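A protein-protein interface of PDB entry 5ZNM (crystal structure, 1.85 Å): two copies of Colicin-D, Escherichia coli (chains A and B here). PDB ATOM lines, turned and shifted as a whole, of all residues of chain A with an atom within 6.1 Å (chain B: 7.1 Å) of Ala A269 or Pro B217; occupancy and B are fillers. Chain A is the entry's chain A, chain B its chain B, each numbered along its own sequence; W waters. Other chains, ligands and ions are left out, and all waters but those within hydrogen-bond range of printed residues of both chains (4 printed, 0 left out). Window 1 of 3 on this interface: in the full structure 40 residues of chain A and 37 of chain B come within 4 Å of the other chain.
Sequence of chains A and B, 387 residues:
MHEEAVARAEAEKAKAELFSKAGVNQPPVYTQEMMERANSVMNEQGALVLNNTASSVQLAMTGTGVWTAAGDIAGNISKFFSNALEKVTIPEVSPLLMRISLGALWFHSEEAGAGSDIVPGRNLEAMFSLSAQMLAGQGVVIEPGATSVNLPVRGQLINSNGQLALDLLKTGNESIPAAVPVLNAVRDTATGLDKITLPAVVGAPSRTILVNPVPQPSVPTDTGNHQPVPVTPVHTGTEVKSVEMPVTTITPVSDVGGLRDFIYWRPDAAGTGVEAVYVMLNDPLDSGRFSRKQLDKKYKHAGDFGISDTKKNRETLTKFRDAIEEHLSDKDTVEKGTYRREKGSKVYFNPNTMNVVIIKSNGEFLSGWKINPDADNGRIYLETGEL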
ATOM      1  N   ALA A  54       0.541 -12.679  18.945  1.00  0.00           N
ATOM      2  CA  ALA A  54       0.067 -13.482  20.066  1.00  0.00           C
ATOM      3  C   ALA A  54      -1.266 -12.962  20.595  1.00  0.00           C
ATOM      4  O   ALA A  54      -1.516 -11.751  20.616  1.00  0.00           O
ATOM      5  CB  ALA A  54       1.102 -13.496  21.190  1.00  0.00           C
ATOM      6  N   SER A  55      -2.120 -13.895  21.025  1.00  0.00           N
ATOM      7  CA  SER A  55      -3.387 -13.569  21.682  1.00  0.00           C
ATOM      8  C   SER A  55      -4.312 -12.764  20.776  1.00  0.00           C
ATOM      9  O   SER A  55      -5.057 -11.909  21.239  1.00  0.00           O
ATOM     10  CB  SER A  55      -3.158 -12.816  22.999  1.00  0.00           C
ATOM     11  OG  SER A  55      -2.460 -13.638  23.925  1.00  0.00           O
ATOM     12  N   ALA A  70      -6.486  -7.465  18.646  1.00  0.00           N
ATOM     13  CA  ALA A  70      -5.771  -7.877  19.837  1.00  0.00           C
ATOM     14  C   ALA A  70      -6.035  -6.862  20.939  1.00  0.00           C
ATOM     15  O   ALA A  70      -6.363  -5.705  20.672  1.00  0.00           O
ATOM     16  CB  ALA A  70      -4.259  -8.020  19.577  1.00  0.00           C
ATOM     17  N   GLY A  71      -5.919  -7.319  22.171  1.00  0.00           N
ATOM     18  CA  GLY A  71      -6.205  -6.485  23.313  1.00  0.00           C
ATOM     19  C   GLY A  71      -7.577  -6.763  23.886  1.00  0.00           C
ATOM     20  O   GLY A  71      -8.295  -7.688  23.506  1.00  0.00           O
ATOM     21  N   ASP A  72      -7.949  -5.914  24.826  1.00  0.00           N
ATOM     22  CA  ASP A  72      -9.214  -6.117  25.498  1.00  0.00           C
ATOM     23  C   ASP A  72     -10.356  -5.831  24.539  1.00  0.00           C
ATOM     24  O   ASP A  72     -11.375  -6.537  24.541  1.00  0.00           O
ATOM     25  CB  ASP A  72      -9.207  -5.241  26.740  1.00  0.00           C
ATOM     26  CG  ASP A  72      -7.807  -5.174  27.364  1.00  0.00           C
ATOM     27  OD1 ASP A  72      -7.191  -6.241  27.590  1.00  0.00           O
ATOM     28  OD2 ASP A  72      -7.282  -4.068  27.553  1.00  0.00           O
ATOM     29  N   PRO A 267       4.200 -18.961  19.408  1.00  0.00           N
ATOM     30  CA  PRO A 267       4.786 -18.409  20.635  1.00  0.00           C
ATOM     31  C   PRO A 267       3.805 -17.477  21.330  1.00  0.00           C
ATOM     32  O   PRO A 267       2.946 -16.847  20.698  1.00  0.00           O
ATOM     33  CB  PRO A 267       6.029 -17.658  20.140  1.00  0.00           C
ATOM     34  CG  PRO A 267       6.402 -18.324  18.843  1.00  0.00           C
ATOM     35  CD  PRO A 267       5.043 -18.694  18.228  1.00  0.00           C
ATOM     36  N   ASP A 268       3.917 -17.414  22.657  1.00  0.00           N
ATOM     37  CA  ASP A 268       3.087 -16.484  23.404  1.00  0.00           C
ATOM     38  C   ASP A 268       3.635 -15.061  23.278  1.00  0.00           C
ATOM     39  O   ASP A 268       4.624 -14.797  22.583  1.00  0.00           O
ATOM     40  CB  ASP A 268       2.948 -16.929  24.863  1.00  0.00           C
ATOM     41  CG  ASP A 268       4.283 -16.980  25.615  1.00  0.00           C
ATOM     42  OD1 ASP A 268       5.309 -16.497  25.102  1.00  0.00           O
ATOM     43  OD2 ASP A 268       4.286 -17.520  26.739  1.00  0.00           O
ATOM     44  N   ALA A 269       2.942 -14.118  23.922  1.00  0.00           N
ATOM     45  CA  ALA A 269       3.294 -12.705  23.768  1.00  0.00           C
ATOM     46  C   ALA A 269       4.724 -12.424  24.234  1.00  0.00           C
ATOM     47  O   ALA A 269       5.445 -11.634  23.609  1.00  0.00           O
ATOM     48  CB  ALA A 269       2.284 -11.831  24.524  1.00  0.00           C
ATOM     49  N   ALA A 270       5.148 -13.054  25.335  1.00  0.00           N
ATOM     50  CA  ALA A 270       6.513 -12.907  25.824  1.00  0.00           C
ATOM     51  C   ALA A 270       7.530 -13.537  24.885  1.00  0.00           C
ATOM     52  O   ALA A 270       8.705 -13.163  24.926  1.00  0.00           O
ATOM     53  CB  ALA A 270       6.642 -13.539  27.215  1.00  0.00           C
ATOM     54  N   GLY A 271       7.100 -14.478  24.048  1.00  0.00           N
ATOM     55  CA  GLY A 271       7.969 -15.164  23.120  1.00  0.00           C
ATOM     56  C   GLY A 271       8.718 -16.336  23.707  1.00  0.00           C
ATOM     57  O   GLY A 271       9.478 -16.988  22.978  1.00  0.00           O
ATOM     58  N   THR A 272       8.524 -16.635  24.995  1.00  0.00           N
ATOM     59  CA  THR A 272       9.253 -17.694  25.683  1.00  0.00           C
ATOM     60  C   THR A 272       8.385 -18.896  26.009  1.00  0.00           C
ATOM     61  O   THR A 272       8.902 -19.903  26.505  1.00  0.00           O
ATOM     62  CB  THR A 272       9.874 -17.145  26.978  1.00  0.00           C
ATOM     63  OG1 THR A 272       8.845 -16.547  27.782  1.00  0.00           O
ATOM     64  CG2 THR A 272      10.932 -16.105  26.636  1.00  0.00           C
ATOM     65  N   GLY A 273       7.082 -18.807  25.764  1.00  0.00           N
ATOM     66  CA  GLY A 273       6.161 -19.909  25.951  1.00  0.00           C
ATOM     67  C   GLY A 273       5.284 -20.059  24.718  1.00  0.00           C
ATOM     68  O   GLY A 273       5.623 -19.519  23.661  1.00  0.00           O
ATOM     69  N   GLU A 275       1.088 -20.749  22.889  1.00  0.00           N
ATOM     70  CA  GLU A 275      -0.359 -20.634  23.014  1.00  0.00           C
ATOM     71  C   GLU A 275      -1.026 -21.352  21.856  1.00  0.00           C
ATOM     72  O   GLU A 275      -0.547 -21.296  20.719  1.00  0.00           O
ATOM     73  CB  GLU A 275      -0.831 -19.166  23.048  1.00  0.00           C
ATOM     74  CG  GLU A 275      -0.378 -18.330  21.890  1.00  0.00           C
ATOM     75  CD  GLU A 275      -0.997 -16.932  21.899  1.00  0.00           C
ATOM     76  OE1 GLU A 275      -1.130 -16.321  22.990  1.00  0.00           O
ATOM     77  OE2 GLU A 275      -1.338 -16.444  20.810  1.00  0.00           O
ATOM     78  N   ASN B  51       2.491  -0.689  28.982  1.00  0.00           N
ATOM     79  CA  ASN B  51       2.930  -1.983  28.463  1.00  0.00           C
ATOM     80  C   ASN B  51       3.686  -1.792  27.157  1.00  0.00           C
ATOM     81  O   ASN B  51       3.295  -0.975  26.329  1.00  0.00           O
ATOM     82  CB  ASN B  51       1.744  -2.920  28.218  1.00  0.00           C
ATOM     83  CG  ASN B  51       1.034  -3.313  29.491  1.00  0.00           C
ATOM     84  OD1 ASN B  51       1.616  -3.281  30.580  1.00  0.00           O
ATOM     85  ND2 ASN B  51      -0.235  -3.679  29.366  1.00  0.00           N
ATOM     86  N   THR B  53       3.564  -3.615  24.649  1.00  0.00           N
ATOM     87  CA  THR B  53       2.846  -4.245  23.549  1.00  0.00           C
ATOM     88  C   THR B  53       2.992  -3.399  22.287  1.00  0.00           C
ATOM     89  O   THR B  53       2.512  -2.268  22.240  1.00  0.00           O
ATOM     90  CB  THR B  53       1.374  -4.371  23.924  1.00  0.00           C
ATOM     91  OG1 THR B  53       1.273  -4.933  25.235  1.00  0.00           O
ATOM     92  CG2 THR B  53       0.632  -5.255  22.918  1.00  0.00           C
ATOM     93  N   ALA B  54       3.639  -3.943  21.259  1.00  0.00           N
ATOM     94  CA  ALA B  54       4.001  -3.125  20.105  1.00  0.00           C
ATOM     95  C   ALA B  54       2.775  -2.687  19.301  1.00  0.00           C
ATOM     96  O   ALA B  54       1.797  -3.428  19.171  1.00  0.00           O
ATOM     97  CB  ALA B  54       4.972  -3.887  19.196  1.00  0.00           C
ATOM     98  N   SER B  56       0.389  -0.592  19.837  1.00  0.00           N
ATOM     99  CA  SER B  56      -0.859  -0.632  20.573  1.00  0.00           C
ATOM    100  C   SER B  56      -1.256   0.769  21.014  1.00  0.00           C
ATOM    101  O   SER B  56      -0.422   1.671  21.135  1.00  0.00           O
ATOM    102  CB  SER B  56      -0.757  -1.561  21.790  1.00  0.00           C
ATOM    103  OG  SER B  56       0.255  -1.123  22.690  1.00  0.00           O
ATOM    104  N   VAL B  66      -4.946  -1.187  32.881  1.00  0.00           N
ATOM    105  CA  VAL B  66      -4.599  -0.785  31.523  1.00  0.00           C
ATOM    106  C   VAL B  66      -5.574  -1.430  30.546  1.00  0.00           C
ATOM    107  O   VAL B  66      -5.794  -2.644  30.586  1.00  0.00           O
ATOM    108  CB  VAL B  66      -3.151  -1.170  31.168  1.00  0.00           C
ATOM    109  CG1 VAL B  66      -2.838  -0.768  29.727  1.00  0.00           C
ATOM    110  CG2 VAL B  66      -2.160  -0.521  32.152  1.00  0.00           C
ATOM    111  N   TRP B  67      -6.142  -0.611  29.669  1.00  0.00           N
ATOM    112  CA  TRP B  67      -6.918  -1.057  28.527  1.00  0.00           C
ATOM    113  C   TRP B  67      -6.036  -0.963  27.294  1.00  0.00           C
ATOM    114  O   TRP B  67      -5.292   0.014  27.130  1.00  0.00           O
ATOM    115  CB  TRP B  67      -8.153  -0.175  28.380  1.00  0.00           C
ATOM    116  CG  TRP B  67      -8.999  -0.426  27.159  1.00  0.00           C
ATOM    117  CD1 TRP B  67     -10.091  -1.241  27.077  1.00  0.00           C
ATOM    118  CD2 TRP B  67      -8.862   0.193  25.880  1.00  0.00           C
ATOM    119  NE1 TRP B  67     -10.636  -1.176  25.820  1.00  0.00           N
ATOM    120  CE2 TRP B  67      -9.898  -0.304  25.063  1.00  0.00           C
ATOM    121  CE3 TRP B  67      -7.959   1.113  25.339  1.00  0.00           C
ATOM    122  CZ2 TRP B  67     -10.050   0.076  23.732  1.00  0.00           C
ATOM    123  CZ3 TRP B  67      -8.114   1.499  24.021  1.00  0.00           C
ATOM    124  CH2 TRP B  67      -9.155   0.981  23.231  1.00  0.00           C
ATOM    125  N   THR B  68      -6.107  -1.979  26.439  1.00  0.00           N
ATOM    126  CA  THR B  68      -5.209  -2.118  25.296  1.00  0.00           C
ATOM    127  C   THR B  68      -6.011  -2.365  24.021  1.00  0.00           C
ATOM    128  O   THR B  68      -6.987  -3.119  24.031  1.00  0.00           O
ATOM    129  CB  THR B  68      -4.214  -3.295  25.524  1.00  0.00           C
ATOM    130  OG1 THR B  68      -3.419  -3.038  26.693  1.00  0.00           O
ATOM    131  CG2 THR B  68      -3.288  -3.467  24.320  1.00  0.00           C
ATOM    132  N   ALA B  69      -5.600  -1.730  22.922  1.00  0.00           N
ATOM    133  CA  ALA B  69      -6.137  -2.044  21.605  1.00  0.00           C
ATOM    134  C   ALA B  69      -4.984  -2.137  20.619  1.00  0.00           C
ATOM    135  O   ALA B  69      -4.124  -1.251  20.579  1.00  0.00           O
ATOM    136  CB  ALA B  69      -7.154  -1.002  21.132  1.00  0.00           C
ATOM    137  N   ALA B  70      -4.957  -3.217  19.842  1.00  0.00           N
ATOM    138  CA  ALA B  70      -3.962  -3.382  18.800  1.00  0.00           C
ATOM    139  C   ALA B  70      -4.618  -4.075  17.611  1.00  0.00           C
ATOM    140  O   ALA B  70      -5.658  -4.729  17.742  1.00  0.00           O
ATOM    141  CB  ALA B  70      -2.752  -4.182  19.301  1.00  0.00           C
ATOM    142  N   VAL B 214       7.507  -6.565  28.898  1.00  0.00           N
ATOM    143  CA  VAL B 214       7.087  -7.781  28.212  1.00  0.00           C
ATOM    144  C   VAL B 214       5.792  -7.484  27.456  1.00  0.00           C
ATOM    145  O   VAL B 214       4.796  -7.111  28.096  1.00  0.00           O
ATOM    146  CB  VAL B 214       6.879  -8.936  29.197  1.00  0.00           C
ATOM    147  CG1 VAL B 214       6.331 -10.150  28.457  1.00  0.00           C
ATOM    148  CG2 VAL B 214       8.189  -9.277  29.908  1.00  0.00           C
ATOM    149  N   PRO B 215       5.755  -7.668  26.138  1.00  0.00           N
ATOM    150  CA  PRO B 215       4.497  -7.490  25.396  1.00  0.00           C
ATOM    151  C   PRO B 215       3.380  -8.292  26.038  1.00  0.00           C
ATOM    152  O   PRO B 215       3.557  -9.457  26.400  1.00  0.00           O
ATOM    153  CB  PRO B 215       4.830  -8.023  23.992  1.00  0.00           C
ATOM    154  CG  PRO B 215       6.336  -7.878  23.880  1.00  0.00           C
ATOM    155  CD  PRO B 215       6.845  -8.170  25.277  1.00  0.00           C
ATOM    156  N   GLN B 216       2.219  -7.662  26.206  1.00  0.00           N
ATOM    157  CA  GLN B 216       1.113  -8.279  26.939  1.00  0.00           C
ATOM    158  C   GLN B 216      -0.205  -7.702  26.455  1.00  0.00           C
ATOM    159  O   GLN B 216      -0.850  -6.904  27.150  1.00  0.00           O
ATOM    160  CB  GLN B 216       1.280  -8.056  28.435  1.00  0.00           C
ATOM    161  CG  GLN B 216       0.545  -9.063  29.293  1.00  0.00           C
ATOM    162  CD  GLN B 216       1.092  -9.053  30.710  1.00  0.00           C
ATOM    163  OE1 GLN B 216       0.593  -8.320  31.566  1.00  0.00           O
ATOM    164  NE2 GLN B 216       2.151  -9.841  30.951  1.00  0.00           N
ATOM    165  N   PRO B 217      -0.643  -8.087  25.252  1.00  0.00           N
ATOM    166  CA  PRO B 217      -1.958  -7.613  24.775  1.00  0.00           C
ATOM    167  C   PRO B 217      -3.103  -8.066  25.662  1.00  0.00           C
ATOM    168  O   PRO B 217      -4.133  -7.375  25.756  1.00  0.00           O
ATOM    169  CB  PRO B 217      -2.052  -8.219  23.367  1.00  0.00           C
ATOM    170  CG  PRO B 217      -1.150  -9.420  23.426  1.00  0.00           C
ATOM    171  CD  PRO B 217      -0.001  -8.981  24.281  1.00  0.00           C
ATOM    172  N   SER B 218      -2.964  -9.228  26.291  1.00  0.00           N
ATOM    173  CA  SER B 218      -3.845  -9.640  27.369  1.00  0.00           C
ATOM    174  C   SER B 218      -3.047 -10.547  28.295  1.00  0.00           C
ATOM    175  O   SER B 218      -1.919 -10.944  27.990  1.00  0.00           O
ATOM    176  CB  SER B 218      -5.106 -10.329  26.841  1.00  0.00           C
ATOM    177  OG  SER B 218      -4.794 -11.207  25.785  1.00  0.00           O
ATOM    178  N   VAL B 219      -3.648 -10.863  29.430  1.00  0.00           N
ATOM    179  CA  VAL B 219      -2.974 -11.650  30.470  1.00  0.00           C
ATOM    180  C   VAL B 219      -2.850 -13.096  30.007  1.00  0.00           C
ATOM    181  O   VAL B 219      -3.858 -13.702  29.599  1.00  0.00           O
ATOM    182  CB  VAL B 219      -3.754 -11.565  31.784  1.00  0.00           C
ATOM    183  CG1 VAL B 219      -3.178 -12.537  32.815  1.00  0.00           C
ATOM    184  CG2 VAL B 219      -3.753 -10.142  32.306  1.00  0.00           C
ATOM    185  N   PRO B 220      -1.663 -13.695  30.054  1.00  0.00           N
ATOM    186  CA  PRO B 220      -1.556 -15.130  29.747  1.00  0.00           C
ATOM    187  C   PRO B 220      -2.224 -15.961  30.834  1.00  0.00           C
ATOM    188  O   PRO B 220      -2.018 -15.722  32.024  1.00  0.00           O
ATOM    189  CB  PRO B 220      -0.043 -15.379  29.688  1.00  0.00           C
ATOM    190  CG  PRO B 220       0.582 -14.199  30.407  1.00  0.00           C
ATOM    191  CD  PRO B 220      -0.352 -13.044  30.237  1.00  0.00           C
ATOM    192  N   HIS B 226       3.561 -21.111  29.885  1.00  0.00           N
ATOM    193  CA  HIS B 226       4.185 -19.798  29.902  1.00  0.00           C
ATOM    194  C   HIS B 226       5.255 -19.761  30.981  1.00  0.00           C
ATOM    195  O   HIS B 226       5.188 -20.500  31.959  1.00  0.00           O
ATOM    196  CB  HIS B 226       3.164 -18.694  30.176  1.00  0.00           C
ATOM    197  CG  HIS B 226       1.973 -18.741  29.278  1.00  0.00           C
ATOM    198  ND1 HIS B 226       2.020 -18.329  27.966  1.00  0.00           N
ATOM    199  CD2 HIS B 226       0.699 -19.144  29.504  1.00  0.00           C
ATOM    200  CE1 HIS B 226       0.828 -18.486  27.416  1.00  0.00           C
ATOM    201  NE2 HIS B 226       0.008 -18.972  28.330  1.00  0.00           N
ATOM    202  N   VAL B 234      -5.229  -5.252  34.383  1.00  0.00           N
ATOM    203  CA  VAL B 234      -6.000  -4.949  33.185  1.00  0.00           C
ATOM    204  C   VAL B 234      -7.251  -4.170  33.568  1.00  0.00           C
ATOM    205  O   VAL B 234      -7.833  -4.359  34.644  1.00  0.00           O
ATOM    206  CB  VAL B 234      -6.342  -6.239  32.410  1.00  0.00           C
ATOM    207  CG1 VAL B 234      -7.276  -5.960  31.239  1.00  0.00           C
ATOM    208  CG2 VAL B 234      -5.062  -6.886  31.904  1.00  0.00           C
HETATM  209  O   HOH W   1     -11.940  -3.850  25.958  1.00  0.00           O
HETATM  210  O   HOH W   2      -0.867 -12.299  25.827  1.00  0.00           O
HETATM  211  O   HOH W   3      -5.174  -9.864  23.001  1.00  0.00           O
HETATM  212  O   HOH W   4      -4.440  -4.115  28.725  1.00  0.00           O
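The backbone NH (N) of Ala A270 sits close to the side-chain carboxylate (OD1) of Asp A268, at 3.5 Å.
The side-chain carboxylate (OE2) of Glu A275 sits at hydrogen-bond distance from the backbone NH (N) of Ser A55.
N of Asp A268 is in hydrogen-bond range of O of Gly A273, 2.9 Å away.
The side-chain carboxylate of Asp A268 sits at hydrogen-bond distance from the backbone NH of Thr A272 (3.2 Å).
The side-chain carboxylate (OD1) of Asp A268 is in hydrogen-bond range of the backbone NH (N) of Gly A271, at 2.9 Å.
Ala A70 touches its own counterpart, Ala B70.
Positions printed for both chains: 54 and 70.
Of the 16 pairs that touch across the chains among the printed residues, 1 has its exchanged pair printed and touching as well.
OD2 of Asp A268 sits at hydrogen-bond distance from ND1 of His B226, at 2.7 Å.
The backbone carbonyl oxygen (O) of Ala A70 lies within hydrogen-bond range of the backbone NH (N) of Ala B70.
N of Thr B68 is in hydrogen-bond range of OD2 of Asp A72 (2.6 Å).
Pro B217 touches Ala A54.
CB of Ser A55 touches OG of Ser B218 (3.6 Å).
CA of Ala B69 touches O of Ala A70, 3.8 Å away.
Gly A71 touches Thr B68.
Val B66 touches Asp A72.
Trp B67 touches Asp A72 (CA to OD2, 3.2 Å).
Asp A72 touches Pro B217.
Asp A72 touches Val B234.
Ala A269 touches Pro B215.
Ala A270 touches Val B214 (CB to CG1, 3.6 Å).
Of the printed residues of chain B, Ala A54 touches Pro B217.
Of the printed residues of chain B, Ala A70 touches Ala B69 and Ala B70.
Of the printed residues of chain B, Gly A71 touches Thr B68 (3.5 Å) and Pro B217 (3.3 Å).
Of chain B, only Pro B215 and Pro B217 come within 4 Å of Ala A269.
Printed residues of chain A within 4 Å of Val B214: Ala A270.
Of the printed residues of chain A, Pro B217 touches Ala A54 (3.7 Å), Ser A55 (3.97 Å), Gly A71 (3.3 Å), Asp A72 (3.7 Å) and Ala A269 (3.7 Å).
The nearest residue of chain B that does not touch Ala A269 is Gln B216 (4.5 Å).
Water W4 lies within hydrogen-bond range of the side-chain hydroxyl (OG1) of Thr B68, the backbone carbonyl oxygen (O) of Val B66 and the side-chain carboxylate (OD2) of Asp A72.
Water W3 lies within hydrogen-bond range of the backbone carbonyl oxygen (O) of Ser A55 (2.7 Å), the backbone NH (N) of Gly A71 (2.8 Å) and the side-chain hydroxyl (OG) of Ser B218 (3.1 Å).
Water W2 lies within hydrogen-bond range of O of Ser B218 (2.8 Å) and OG of Ser A55 (2.8 Å).
Water W1 bridges the indole nitrogen (NE1) of Trp B67 (3.0 Å) and the backbone carbonyl oxygen (O) of Asp A72 (3.1 Å).
Of the 18 printed residues of chain B, 11 touch a printed residue of chain A.
Printed residues of chain B that touch a printed residue of chain A: Val B66, Trp B67, Thr B68, Ala B69, Ala B70, Val B214, Pro B215, Pro B217, Ser B218, His B226 and Val B234.
Printed residues of chain A that touch a printed residue of chain B: Ala A54, Ser A55, Ala A70, Gly A71, Asp A72, Asp A268, Ala A269 and Ala A270.
Hydrophobic or aromatic side chains of chain A that line the printed part of chain B: Ala A269 and Ala A270.
Among the printed residues, no Asp or Glu carboxylate lies within 4 Å of a Lys or Arg side-chain nitrogen of the other chain.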
